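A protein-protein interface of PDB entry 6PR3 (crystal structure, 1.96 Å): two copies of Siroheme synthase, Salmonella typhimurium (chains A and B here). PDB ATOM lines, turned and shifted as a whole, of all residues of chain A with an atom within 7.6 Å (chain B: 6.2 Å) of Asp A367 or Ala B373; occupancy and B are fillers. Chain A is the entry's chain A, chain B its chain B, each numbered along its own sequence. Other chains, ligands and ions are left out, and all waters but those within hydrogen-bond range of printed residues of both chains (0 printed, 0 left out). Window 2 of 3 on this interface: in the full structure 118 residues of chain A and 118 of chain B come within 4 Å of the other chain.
O of Asn B370 sits at hydrogen-bond distance from ND2 of Asn A370 (3.1 Å).
NH2 of Arg B354 is in hydrogen-bond range of OD1 of Asn A370 (2.7 Å).
NH2 of Arg A354 lies close to NH2 of Arg B354, at 3.1 Å.
The guanidinium group (NH2) of Arg B354 lies within hydrogen-bond range of the side-chain amide oxygen (OE1) of Gln B376 (2.9 Å).
The backbone carbonyl oxygen (O) of Leu A371 sits at hydrogen-bond distance from the side-chain amide nitrogen (NE2) of Gln A376, at 3.1 Å.
The backbone carbonyl oxygen of Asn B370 lies within hydrogen-bond range of the side-chain amide nitrogen of Gln B376 (3.1 Å).
OD2 of Asp A367 sits close to ND2 of Asn A370 (3.3 Å).
O of Asn A370 sits at hydrogen-bond distance from NE2 of Gln A376 (3.2 Å).
N of Gln B351 lies within hydrogen-bond range of O of Lys B375 (2.9 Å).
OE1 of Gln B376 touches NH1 of Arg A354, at 3.7 Å.
CA of Val A356 touches O of Gln B351, 3.7 Å away.
CD2 of Leu A360 touches NE2 of Gln B351 (3.2 Å).
Gln B351 touches Glu A365 (OE1 to O, 3.7 Å).
CD2 of Leu A366 touches OE1 of Gln B351, at 3.8 Å.
Asp A367 touches Ala B373 (OD2 to CB, 3.7 Å).
Ala B373 touches Asn A370.
OD1 of Asn B370 touches CB of Ala A373, at 3.1 Å.
Arg B354 touches Gln A376 (NH1 to OE1, 3.6 Å).
Of the printed residues of chain B, Arg A354 touches Arg B354 and Gln B376.
Of the printed residues of chain B, Val A356 touches Gln B351 (3.7 Å).
Of the printed residues of chain B, Leu A366 touches Gln B351.
Of chain B, only Ala B373 (3.7 Å) comes within 4 Å of Asp A367.
Glu A369 touches none of the printed residues of chain B.
Of the printed residues of chain A, Asn B370 touches Asn A370 (3.1 Å) and Ala A373 (3.1 Å).
Leu B394 touches none of the printed residues of chain A.
The nearest residue of chain B that does not touch Asp A367 is Gln B351 (4.3 Å).
Printed residues of chain A that touch a printed residue of chain B: Arg A354, Val A356, Leu A360, Glu A365, Leu A366, Asp A367, Asn A370, Ala A373 and Gln A376.
Of the 15 printed residues of chain B, 5 touch a printed residue of chain A.
Hydrophobic or aromatic side chains of chain B that line the printed part of chain A: Ala B373.
Arg B354 touches its own counterpart, Arg A354.
Asn A370 touches Arg B354, but with the chains exchanged Arg A354 does not touch Asn B370 (4.6 Å).
Asn B370 touches its own counterpart, Asn A370.
Asn A370 touches Ala B373, and with the chains exchanged Ala A373 touches Asn B370.
10 positions are printed for both chains.
Of the 12 pairs that touch across the chains among the printed residues, 6 have their exchanged pair printed and touching as well.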
ATOM      1  N   ARG A 354     -23.493  27.548 -30.424  1.00  0.00           N
ATOM      2  CA  ARG A 354     -22.327  27.007 -29.741  1.00  0.00           C
ATOM      3  C   ARG A 354     -21.077  27.442 -30.496  1.00  0.00           C
ATOM      4  O   ARG A 354     -20.894  27.078 -31.660  1.00  0.00           O
ATOM      5  CB  ARG A 354     -22.428  25.481 -29.667  1.00  0.00           C
ATOM      6  CG  ARG A 354     -21.497  24.863 -28.659  1.00  0.00           C
ATOM      7  CD  ARG A 354     -22.181  24.765 -27.320  1.00  0.00           C
ATOM      8  NE  ARG A 354     -23.169  23.700 -27.326  1.00  0.00           N
ATOM      9  CZ  ARG A 354     -23.004  22.537 -26.714  1.00  0.00           C
ATOM     10  NH1 ARG A 354     -21.892  22.303 -26.027  1.00  0.00           N
ATOM     11  NH2 ARG A 354     -23.960  21.625 -26.770  1.00  0.00           N
ATOM     12  N   VAL A 356     -17.269  26.747 -30.653  1.00  0.00           N
ATOM     13  CA  VAL A 356     -16.487  25.593 -30.217  1.00  0.00           C
ATOM     14  C   VAL A 356     -15.111  25.659 -30.852  1.00  0.00           C
ATOM     15  O   VAL A 356     -14.987  26.000 -32.035  1.00  0.00           O
ATOM     16  CB  VAL A 356     -17.151  24.255 -30.624  1.00  0.00           C
ATOM     17  CG1 VAL A 356     -16.567  23.099 -29.823  1.00  0.00           C
ATOM     18  CG2 VAL A 356     -18.635  24.321 -30.477  1.00  0.00           C
ATOM     19  N   LEU A 360      -7.809  21.203 -29.274  1.00  0.00           N
ATOM     20  CA  LEU A 360      -7.778  21.139 -27.818  1.00  0.00           C
ATOM     21  C   LEU A 360      -6.380  20.832 -27.291  1.00  0.00           C
ATOM     22  O   LEU A 360      -5.506  20.339 -28.012  1.00  0.00           O
ATOM     23  CB  LEU A 360      -8.750  20.074 -27.300  1.00  0.00           C
ATOM     24  CG  LEU A 360     -10.120  20.533 -26.819  1.00  0.00           C
ATOM     25  CD1 LEU A 360     -10.875  21.161 -27.972  1.00  0.00           C
ATOM     26  CD2 LEU A 360     -10.873  19.341 -26.276  1.00  0.00           C
ATOM     27  N   GLU A 365     -10.869  15.897 -25.221  1.00  0.00           N
ATOM     28  CA  GLU A 365     -11.776  15.665 -26.335  1.00  0.00           C
ATOM     29  C   GLU A 365     -13.113  16.328 -26.036  1.00  0.00           C
ATOM     30  O   GLU A 365     -13.523  16.449 -24.877  1.00  0.00           O
ATOM     31  CB  GLU A 365     -11.954  14.157 -26.623  1.00  0.00           C
ATOM     32  CG  GLU A 365     -13.021  13.810 -27.675  1.00  0.00           C
ATOM     33  CD  GLU A 365     -12.581  14.134 -29.107  1.00  0.00           C
ATOM     34  OE1 GLU A 365     -12.339  13.193 -29.896  1.00  0.00           O
ATOM     35  OE2 GLU A 365     -12.485  15.338 -29.444  1.00  0.00           O
ATOM     36  N   LEU A 366     -13.778  16.769 -27.099  1.00  0.00           N
ATOM     37  CA  LEU A 366     -15.050  17.464 -26.998  1.00  0.00           C
ATOM     38  C   LEU A 366     -16.154  16.530 -26.505  1.00  0.00           C
ATOM     39  O   LEU A 366     -16.100  15.304 -26.667  1.00  0.00           O
ATOM     40  CB  LEU A 366     -15.435  18.057 -28.354  1.00  0.00           C
ATOM     41  CG  LEU A 366     -14.472  19.109 -28.917  1.00  0.00           C
ATOM     42  CD1 LEU A 366     -14.889  19.556 -30.318  1.00  0.00           C
ATOM     43  CD2 LEU A 366     -14.389  20.301 -27.980  1.00  0.00           C
ATOM     44  N   ASP A 367     -17.172  17.138 -25.897  1.00  0.00           N
ATOM     45  CA  ASP A 367     -18.342  16.423 -25.386  1.00  0.00           C
ATOM     46  C   ASP A 367     -19.318  16.244 -26.544  1.00  0.00           C
ATOM     47  O   ASP A 367     -20.282  16.994 -26.711  1.00  0.00           O
ATOM     48  CB  ASP A 367     -18.971  17.192 -24.233  1.00  0.00           C
ATOM     49  CG  ASP A 367     -20.152  16.469 -23.620  1.00  0.00           C
ATOM     50  OD1 ASP A 367     -20.316  15.261 -23.883  1.00  0.00           O
ATOM     51  OD2 ASP A 367     -20.918  17.118 -22.874  1.00  0.00           O
ATOM     52  N   TRP A 368     -19.053  15.223 -27.366  1.00  0.00           N
ATOM     53  CA  TRP A 368     -19.781  15.106 -28.625  1.00  0.00           C
ATOM     54  C   TRP A 368     -21.272  14.869 -28.413  1.00  0.00           C
ATOM     55  O   TRP A 368     -22.081  15.337 -29.225  1.00  0.00           O
ATOM     56  CB  TRP A 368     -19.176  13.991 -29.473  1.00  0.00           C
ATOM     57  CG  TRP A 368     -17.793  14.297 -29.903  1.00  0.00           C
ATOM     58  CD1 TRP A 368     -16.648  13.711 -29.460  1.00  0.00           C
ATOM     59  CD2 TRP A 368     -17.398  15.294 -30.855  1.00  0.00           C
ATOM     60  NE1 TRP A 368     -15.558  14.269 -30.092  1.00  0.00           N
ATOM     61  CE2 TRP A 368     -15.993  15.243 -30.953  1.00  0.00           C
ATOM     62  CE3 TRP A 368     -18.101  16.209 -31.651  1.00  0.00           C
ATOM     63  CZ2 TRP A 368     -15.274  16.074 -31.818  1.00  0.00           C
ATOM     64  CZ3 TRP A 368     -17.386  17.043 -32.499  1.00  0.00           C
ATOM     65  CH2 TRP A 368     -15.988  16.970 -32.578  1.00  0.00           C
ATOM     66  N   GLU A 369     -21.649  14.134 -27.352  1.00  0.00           N
ATOM     67  CA  GLU A 369     -23.063  14.007 -26.987  1.00  0.00           C
ATOM     68  C   GLU A 369     -23.713  15.375 -26.909  1.00  0.00           C
ATOM     69  O   GLU A 369     -24.822  15.593 -27.419  1.00  0.00           O
ATOM     70  CB  GLU A 369     -23.240  13.318 -25.629  1.00  0.00           C
ATOM     71  CG  GLU A 369     -22.689  11.933 -25.478  1.00  0.00           C
ATOM     72  CD  GLU A 369     -21.249  11.918 -24.998  1.00  0.00           C
ATOM     73  OE1 GLU A 369     -20.887  10.966 -24.266  1.00  0.00           O
ATOM     74  OE2 GLU A 369     -20.484  12.847 -25.354  1.00  0.00           O
ATOM     75  N   ASN A 370     -23.022  16.308 -26.256  1.00  0.00           N
ATOM     76  CA  ASN A 370     -23.559  17.647 -26.063  1.00  0.00           C
ATOM     77  C   ASN A 370     -23.673  18.388 -27.388  1.00  0.00           C
ATOM     78  O   ASN A 370     -24.691  19.032 -27.666  1.00  0.00           O
ATOM     79  CB  ASN A 370     -22.657  18.406 -25.090  1.00  0.00           C
ATOM     80  CG  ASN A 370     -23.430  19.290 -24.144  1.00  0.00           C
ATOM     81  OD1 ASN A 370     -23.717  20.443 -24.455  1.00  0.00           O
ATOM     82  ND2 ASN A 370     -23.778  18.751 -22.981  1.00  0.00           N
ATOM     83  N   LEU A 371     -22.639  18.307 -28.222  1.00  0.00           N
ATOM     84  CA  LEU A 371     -22.638  19.077 -29.460  1.00  0.00           C
ATOM     85  C   LEU A 371     -23.653  18.553 -30.461  1.00  0.00           C
ATOM     86  O   LEU A 371     -24.099  19.307 -31.327  1.00  0.00           O
ATOM     87  CB  LEU A 371     -21.247  19.046 -30.074  1.00  0.00           C
ATOM     88  CG  LEU A 371     -20.136  19.550 -29.157  1.00  0.00           C
ATOM     89  CD1 LEU A 371     -18.776  19.307 -29.791  1.00  0.00           C
ATOM     90  CD2 LEU A 371     -20.348  21.018 -28.865  1.00  0.00           C
ATOM     91  N   ALA A 372     -24.026  17.283 -30.369  1.00  0.00           N
ATOM     92  CA  ALA A 372     -24.943  16.716 -31.344  1.00  0.00           C
ATOM     93  C   ALA A 372     -26.403  17.099 -31.096  1.00  0.00           C
ATOM     94  O   ALA A 372     -27.252  16.768 -31.933  1.00  0.00           O
ATOM     95  CB  ALA A 372     -24.804  15.189 -31.363  1.00  0.00           C
ATOM     96  N   ALA A 373     -26.704  17.792 -29.992  1.00  0.00           N
ATOM     97  CA  ALA A 373     -28.084  18.110 -29.626  1.00  0.00           C
ATOM     98  C   ALA A 373     -28.795  18.884 -30.731  1.00  0.00           C
ATOM     99  O   ALA A 373     -28.182  19.652 -31.476  1.00  0.00           O
ATOM    100  CB  ALA A 373     -28.122  18.935 -28.341  1.00  0.00           C
ATOM    101  N   GLN A 376     -29.622  23.613 -32.419  1.00  0.00           N
ATOM    102  CA  GLN A 376     -28.555  24.570 -32.191  1.00  0.00           C
ATOM    103  C   GLN A 376     -27.773  24.780 -33.474  1.00  0.00           C
ATOM    104  O   GLN A 376     -27.869  24.015 -34.442  1.00  0.00           O
ATOM    105  CB  GLN A 376     -27.627  24.159 -31.035  1.00  0.00           C
ATOM    106  CG  GLN A 376     -27.177  22.731 -30.979  1.00  0.00           C
ATOM    107  CD  GLN A 376     -26.328  22.451 -29.732  1.00  0.00           C
ATOM    108  OE1 GLN A 376     -26.129  23.328 -28.885  1.00  0.00           O
ATOM    109  NE2 GLN A 376     -25.812  21.232 -29.628  1.00  0.00           N
ATOM    110  N   LEU A 394     -20.055  13.715 -34.869  1.00  0.00           N
ATOM    111  CA  LEU A 394     -21.419  14.237 -34.819  1.00  0.00           C
ATOM    112  C   LEU A 394     -22.417  13.196 -35.319  1.00  0.00           C
ATOM    113  O   LEU A 394     -23.475  12.993 -34.707  1.00  0.00           O
ATOM    114  CB  LEU A 394     -21.535  15.520 -35.631  1.00  0.00           C
ATOM    115  CG  LEU A 394     -20.849  16.756 -35.033  1.00  0.00           C
ATOM    116  CD1 LEU A 394     -20.890  17.913 -36.033  1.00  0.00           C
ATOM    117  CD2 LEU A 394     -21.518  17.150 -33.718  1.00  0.00           C
ATOM    118  N   PHE A 397     -22.948  10.443 -32.680  1.00  0.00           N
ATOM    119  CA  PHE A 397     -23.745  10.867 -31.543  1.00  0.00           C
ATOM    120  C   PHE A 397     -25.096  11.432 -31.956  1.00  0.00           C
ATOM    121  O   PHE A 397     -25.725  12.143 -31.174  1.00  0.00           O
ATOM    122  CB  PHE A 397     -22.941  11.859 -30.700  1.00  0.00           C
ATOM    123  CG  PHE A 397     -21.921  11.183 -29.840  1.00  0.00           C
ATOM    124  CD1 PHE A 397     -20.633  10.985 -30.290  1.00  0.00           C
ATOM    125  CD2 PHE A 397     -22.272  10.693 -28.593  1.00  0.00           C
ATOM    126  CE1 PHE A 397     -19.704  10.333 -29.492  1.00  0.00           C
ATOM    127  CE2 PHE A 397     -21.348  10.040 -27.798  1.00  0.00           C
ATOM    128  CZ  PHE A 397     -20.070   9.862 -28.245  1.00  0.00           C
ATOM    129  N   GLN B 351     -14.289  24.657 -23.428  1.00  0.00           N
ATOM    130  CA  GLN B 351     -14.089  24.244 -24.809  1.00  0.00           C
ATOM    131  C   GLN B 351     -15.079  24.919 -25.740  1.00  0.00           C
ATOM    132  O   GLN B 351     -14.849  24.965 -26.954  1.00  0.00           O
ATOM    133  CB  GLN B 351     -14.184  22.712 -24.911  1.00  0.00           C
ATOM    134  CG  GLN B 351     -13.106  21.993 -24.089  1.00  0.00           C
ATOM    135  CD  GLN B 351     -13.330  20.487 -23.950  1.00  0.00           C
ATOM    136  OE1 GLN B 351     -14.412  19.970 -24.233  1.00  0.00           O
ATOM    137  NE2 GLN B 351     -12.308  19.785 -23.474  1.00  0.00           N
ATOM    138  N   ARG B 354     -21.770  28.826 -25.147  1.00  0.00           N
ATOM    139  CA  ARG B 354     -23.141  28.644 -25.583  1.00  0.00           C
ATOM    140  C   ARG B 354     -23.903  29.942 -25.385  1.00  0.00           C
ATOM    141  O   ARG B 354     -23.964  30.464 -24.261  1.00  0.00           O
ATOM    142  CB  ARG B 354     -23.826  27.511 -24.831  1.00  0.00           C
ATOM    143  CG  ARG B 354     -25.086  27.074 -25.552  1.00  0.00           C
ATOM    144  CD  ARG B 354     -25.985  26.287 -24.652  1.00  0.00           C
ATOM    145  NE  ARG B 354     -25.321  25.070 -24.225  1.00  0.00           N
ATOM    146  CZ  ARG B 354     -25.691  23.849 -24.582  1.00  0.00           C
ATOM    147  NH1 ARG B 354     -26.750  23.672 -25.365  1.00  0.00           N
ATOM    148  NH2 ARG B 354     -25.001  22.814 -24.131  1.00  0.00           N
ATOM    149  N   TRP B 368     -31.782  20.630 -20.190  1.00  0.00           N
ATOM    150  CA  TRP B 368     -31.077  20.957 -18.953  1.00  0.00           C
ATOM    151  C   TRP B 368     -29.854  20.065 -18.741  1.00  0.00           C
ATOM    152  O   TRP B 368     -28.794  20.550 -18.313  1.00  0.00           O
ATOM    153  CB  TRP B 368     -32.044  20.870 -17.780  1.00  0.00           C
ATOM    154  CG  TRP B 368     -33.003  22.014 -17.771  1.00  0.00           C
ATOM    155  CD1 TRP B 368     -34.361  21.951 -17.908  1.00  0.00           C
ATOM    156  CD2 TRP B 368     -32.676  23.400 -17.639  1.00  0.00           C
ATOM    157  NE1 TRP B 368     -34.899  23.213 -17.858  1.00  0.00           N
ATOM    158  CE2 TRP B 368     -33.886  24.121 -17.692  1.00  0.00           C
ATOM    159  CE3 TRP B 368     -31.477  24.102 -17.474  1.00  0.00           C
ATOM    160  CZ2 TRP B 368     -33.931  25.510 -17.585  1.00  0.00           C
ATOM    161  CZ3 TRP B 368     -31.521  25.482 -17.368  1.00  0.00           C
ATOM    162  CH2 TRP B 368     -32.740  26.172 -17.423  1.00  0.00           C
ATOM    163  N   GLU B 369     -29.979  18.767 -19.040  1.00  0.00           N
ATOM    164  CA  GLU B 369     -28.814  17.886 -19.029  1.00  0.00           C
ATOM    165  C   GLU B 369     -27.668  18.469 -19.846  1.00  0.00           C
ATOM    166  O   GLU B 369     -26.515  18.473 -19.402  1.00  0.00           O
ATOM    167  CB  GLU B 369     -29.199  16.511 -19.571  1.00  0.00           C
ATOM    168  CG  GLU B 369     -28.021  15.689 -20.059  1.00  0.00           C
ATOM    169  CD  GLU B 369     -28.223  14.201 -19.856  1.00  0.00           C
ATOM    170  OE1 GLU B 369     -29.192  13.646 -20.421  1.00  0.00           O
ATOM    171  OE2 GLU B 369     -27.413  13.588 -19.128  1.00  0.00           O
ATOM    172  N   ASN B 370     -27.977  18.992 -21.036  1.00  0.00           N
ATOM    173  CA  ASN B 370     -26.949  19.563 -21.897  1.00  0.00           C
ATOM    174  C   ASN B 370     -26.345  20.810 -21.271  1.00  0.00           C
ATOM    175  O   ASN B 370     -25.120  20.985 -21.270  1.00  0.00           O
ATOM    176  CB  ASN B 370     -27.540  19.891 -23.270  1.00  0.00           C
ATOM    177  CG  ASN B 370     -27.562  18.692 -24.190  1.00  0.00           C
ATOM    178  OD1 ASN B 370     -27.348  18.818 -25.390  1.00  0.00           O
ATOM    179  ND2 ASN B 370     -27.810  17.515 -23.626  1.00  0.00           N
ATOM    180  N   LEU B 371     -27.191  21.684 -20.722  1.00  0.00           N
ATOM    181  CA  LEU B 371     -26.692  22.943 -20.184  1.00  0.00           C
ATOM    182  C   LEU B 371     -25.788  22.719 -18.975  1.00  0.00           C
ATOM    183  O   LEU B 371     -24.889  23.530 -18.723  1.00  0.00           O
ATOM    184  CB  LEU B 371     -27.867  23.853 -19.829  1.00  0.00           C
ATOM    185  CG  LEU B 371     -28.740  24.291 -21.012  1.00  0.00           C
ATOM    186  CD1 LEU B 371     -29.920  25.142 -20.556  1.00  0.00           C
ATOM    187  CD2 LEU B 371     -27.918  25.054 -22.022  1.00  0.00           C
ATOM    188  N   ALA B 372     -25.976  21.613 -18.245  1.00  0.00           N
ATOM    189  CA  ALA B 372     -25.228  21.374 -17.014  1.00  0.00           C
ATOM    190  C   ALA B 372     -23.819  20.837 -17.241  1.00  0.00           C
ATOM    191  O   ALA B 372     -23.055  20.745 -16.271  1.00  0.00           O
ATOM    192  CB  ALA B 372     -25.987  20.399 -16.107  1.00  0.00           C
ATOM    193  N   ALA B 373     -23.450  20.490 -18.472  1.00  0.00           N
ATOM    194  CA  ALA B 373     -22.201  19.770 -18.702  1.00  0.00           C
ATOM    195  C   ALA B 373     -20.991  20.672 -18.467  1.00  0.00           C
ATOM    196  O   ALA B 373     -21.045  21.888 -18.671  1.00  0.00           O
ATOM    197  CB  ALA B 373     -22.164  19.203 -20.124  1.00  0.00           C
ATOM    198  N   GLU B 374     -19.885  20.054 -18.048  1.00  0.00           N
ATOM    199  CA  GLU B 374     -18.679  20.799 -17.712  1.00  0.00           C
ATOM    200  C   GLU B 374     -18.024  21.394 -18.955  1.00  0.00           C
ATOM    201  O   GLU B 374     -18.327  21.032 -20.097  1.00  0.00           O
ATOM    202  CB  GLU B 374     -17.650  19.911 -17.019  1.00  0.00           C
ATOM    203  CG  GLU B 374     -18.168  18.991 -15.948  1.00  0.00           C
ATOM    204  CD  GLU B 374     -17.194  17.854 -15.689  1.00  0.00           C
ATOM    205  OE1 GLU B 374     -15.981  18.134 -15.572  1.00  0.00           O
ATOM    206  OE2 GLU B 374     -17.634  16.686 -15.632  1.00  0.00           O
ATOM    207  N   LYS B 375     -17.078  22.305 -18.705  1.00  0.00           N
ATOM    208  CA  LYS B 375     -16.201  22.856 -19.735  1.00  0.00           C
ATOM    209  C   LYS B 375     -16.953  23.764 -20.697  1.00  0.00           C
ATOM    210  O   LYS B 375     -16.584  23.872 -21.869  1.00  0.00           O
ATOM    211  CB  LYS B 375     -15.478  21.745 -20.513  1.00  0.00           C
ATOM    212  CG  LYS B 375     -14.530  20.919 -19.675  1.00  0.00           C
ATOM    213  CD  LYS B 375     -13.743  21.807 -18.745  1.00  0.00           C
ATOM    214  CE  LYS B 375     -12.261  21.674 -19.010  1.00  0.00           C
ATOM    215  NZ  LYS B 375     -11.462  21.924 -17.775  1.00  0.00           N
ATOM    216  N   GLN B 376     -18.006  24.422 -20.217  1.00  0.00           N
ATOM    217  CA  GLN B 376     -18.750  25.383 -21.011  1.00  0.00           C
ATOM    218  C   GLN B 376     -18.766  26.734 -20.319  1.00  0.00           C
ATOM    219  O   GLN B 376     -18.717  26.823 -19.084  1.00  0.00           O
ATOM    220  CB  GLN B 376     -20.211  24.981 -21.216  1.00  0.00           C
ATOM    221  CG  GLN B 376     -20.491  23.676 -21.896  1.00  0.00           C
ATOM    222  CD  GLN B 376     -21.987  23.440 -21.950  1.00  0.00           C
ATOM    223  OE1 GLN B 376     -22.669  23.966 -22.828  1.00  0.00           O
ATOM    224  NE2 GLN B 376     -22.514  22.687 -20.981  1.00  0.00           N
ATOM    225  N   LEU B 378     -21.734  29.347 -20.304  1.00  0.00           N
ATOM    226  CA  LEU B 378     -23.128  29.579 -20.684  1.00  0.00           C
ATOM    227  C   LEU B 378     -23.432  31.064 -20.620  1.00  0.00           C
ATOM    228  O   LEU B 378     -23.061  31.734 -19.650  1.00  0.00           O
ATOM    229  CB  LEU B 378     -24.107  28.848 -19.768  1.00  0.00           C
ATOM    230  CG  LEU B 378     -23.960  27.352 -19.603  1.00  0.00           C
ATOM    231  CD1 LEU B 378     -24.992  26.844 -18.583  1.00  0.00           C
ATOM    232  CD2 LEU B 378     -24.081  26.648 -20.956  1.00  0.00           C
ATOM    233  N   LEU B 394     -29.831  23.563 -13.113  1.00  0.00           N
ATOM    234  CA  LEU B 394     -28.396  23.305 -13.220  1.00  0.00           C
ATOM    235  C   LEU B 394     -27.887  22.536 -12.001  1.00  0.00           C
ATOM    236  O   LEU B 394     -27.151  21.549 -12.132  1.00  0.00           O
ATOM    237  CB  LEU B 394     -27.635  24.625 -13.407  1.00  0.00           C
ATOM    238  CG  LEU B 394     -27.794  25.308 -14.776  1.00  0.00           C
ATOM    239  CD1 LEU B 394     -27.018  26.636 -14.863  1.00  0.00           C
ATOM    240  CD2 LEU B 394     -27.392  24.375 -15.926  1.00  0.00           C
ATOM    241  N   PHE B 397     -29.065  18.948 -12.135  1.00  0.00           N
ATOM    242  CA  PHE B 397     -28.502  18.107 -13.180  1.00  0.00           C
ATOM    243  C   PHE B 397     -26.990  17.983 -13.059  1.00  0.00           C
ATOM    244  O   PHE B 397     -26.327  17.564 -14.013  1.00  0.00           O
ATOM    245  CB  PHE B 397     -28.916  18.626 -14.558  1.00  0.00           C
ATOM    246  CG  PHE B 397     -30.287  18.175 -14.971  1.00  0.00           C
ATOM    247  CD1 PHE B 397     -31.398  18.969 -14.729  1.00  0.00           C
ATOM    248  CD2 PHE B 397     -30.472  16.936 -15.565  1.00  0.00           C
ATOM    249  CE1 PHE B 397     -32.669  18.548 -15.092  1.00  0.00           C
ATOM    250  CE2 PHE B 397     -31.738  16.505 -15.927  1.00  0.00           C
ATOM    251  CZ  PHE B 397     -32.837  17.313 -15.693  1.00  0.00           C
ATOM    252  N   MET B 399     -24.420  20.314 -12.050  1.00  0.00           N
ATOM    253  CA  MET B 399     -23.438  21.388 -12.052  1.00  0.00           C
ATOM    254  C   MET B 399     -23.035  21.690 -10.613  1.00  0.00           C
ATOM    255  O   MET B 399     -23.895  21.786  -9.731  1.00  0.00           O
ATOM    256  CB  MET B 399     -23.983  22.642 -12.734  1.00  0.00           C
ATOM    257  CG  MET B 399     -22.984  23.795 -12.697  1.00  0.00           C
ATOM    258  SD  MET B 399     -23.447  25.250 -13.652  1.00  0.00           S
ATOM    259  CE  MET B 399     -23.292  24.634 -15.335  1.00  0.00           C
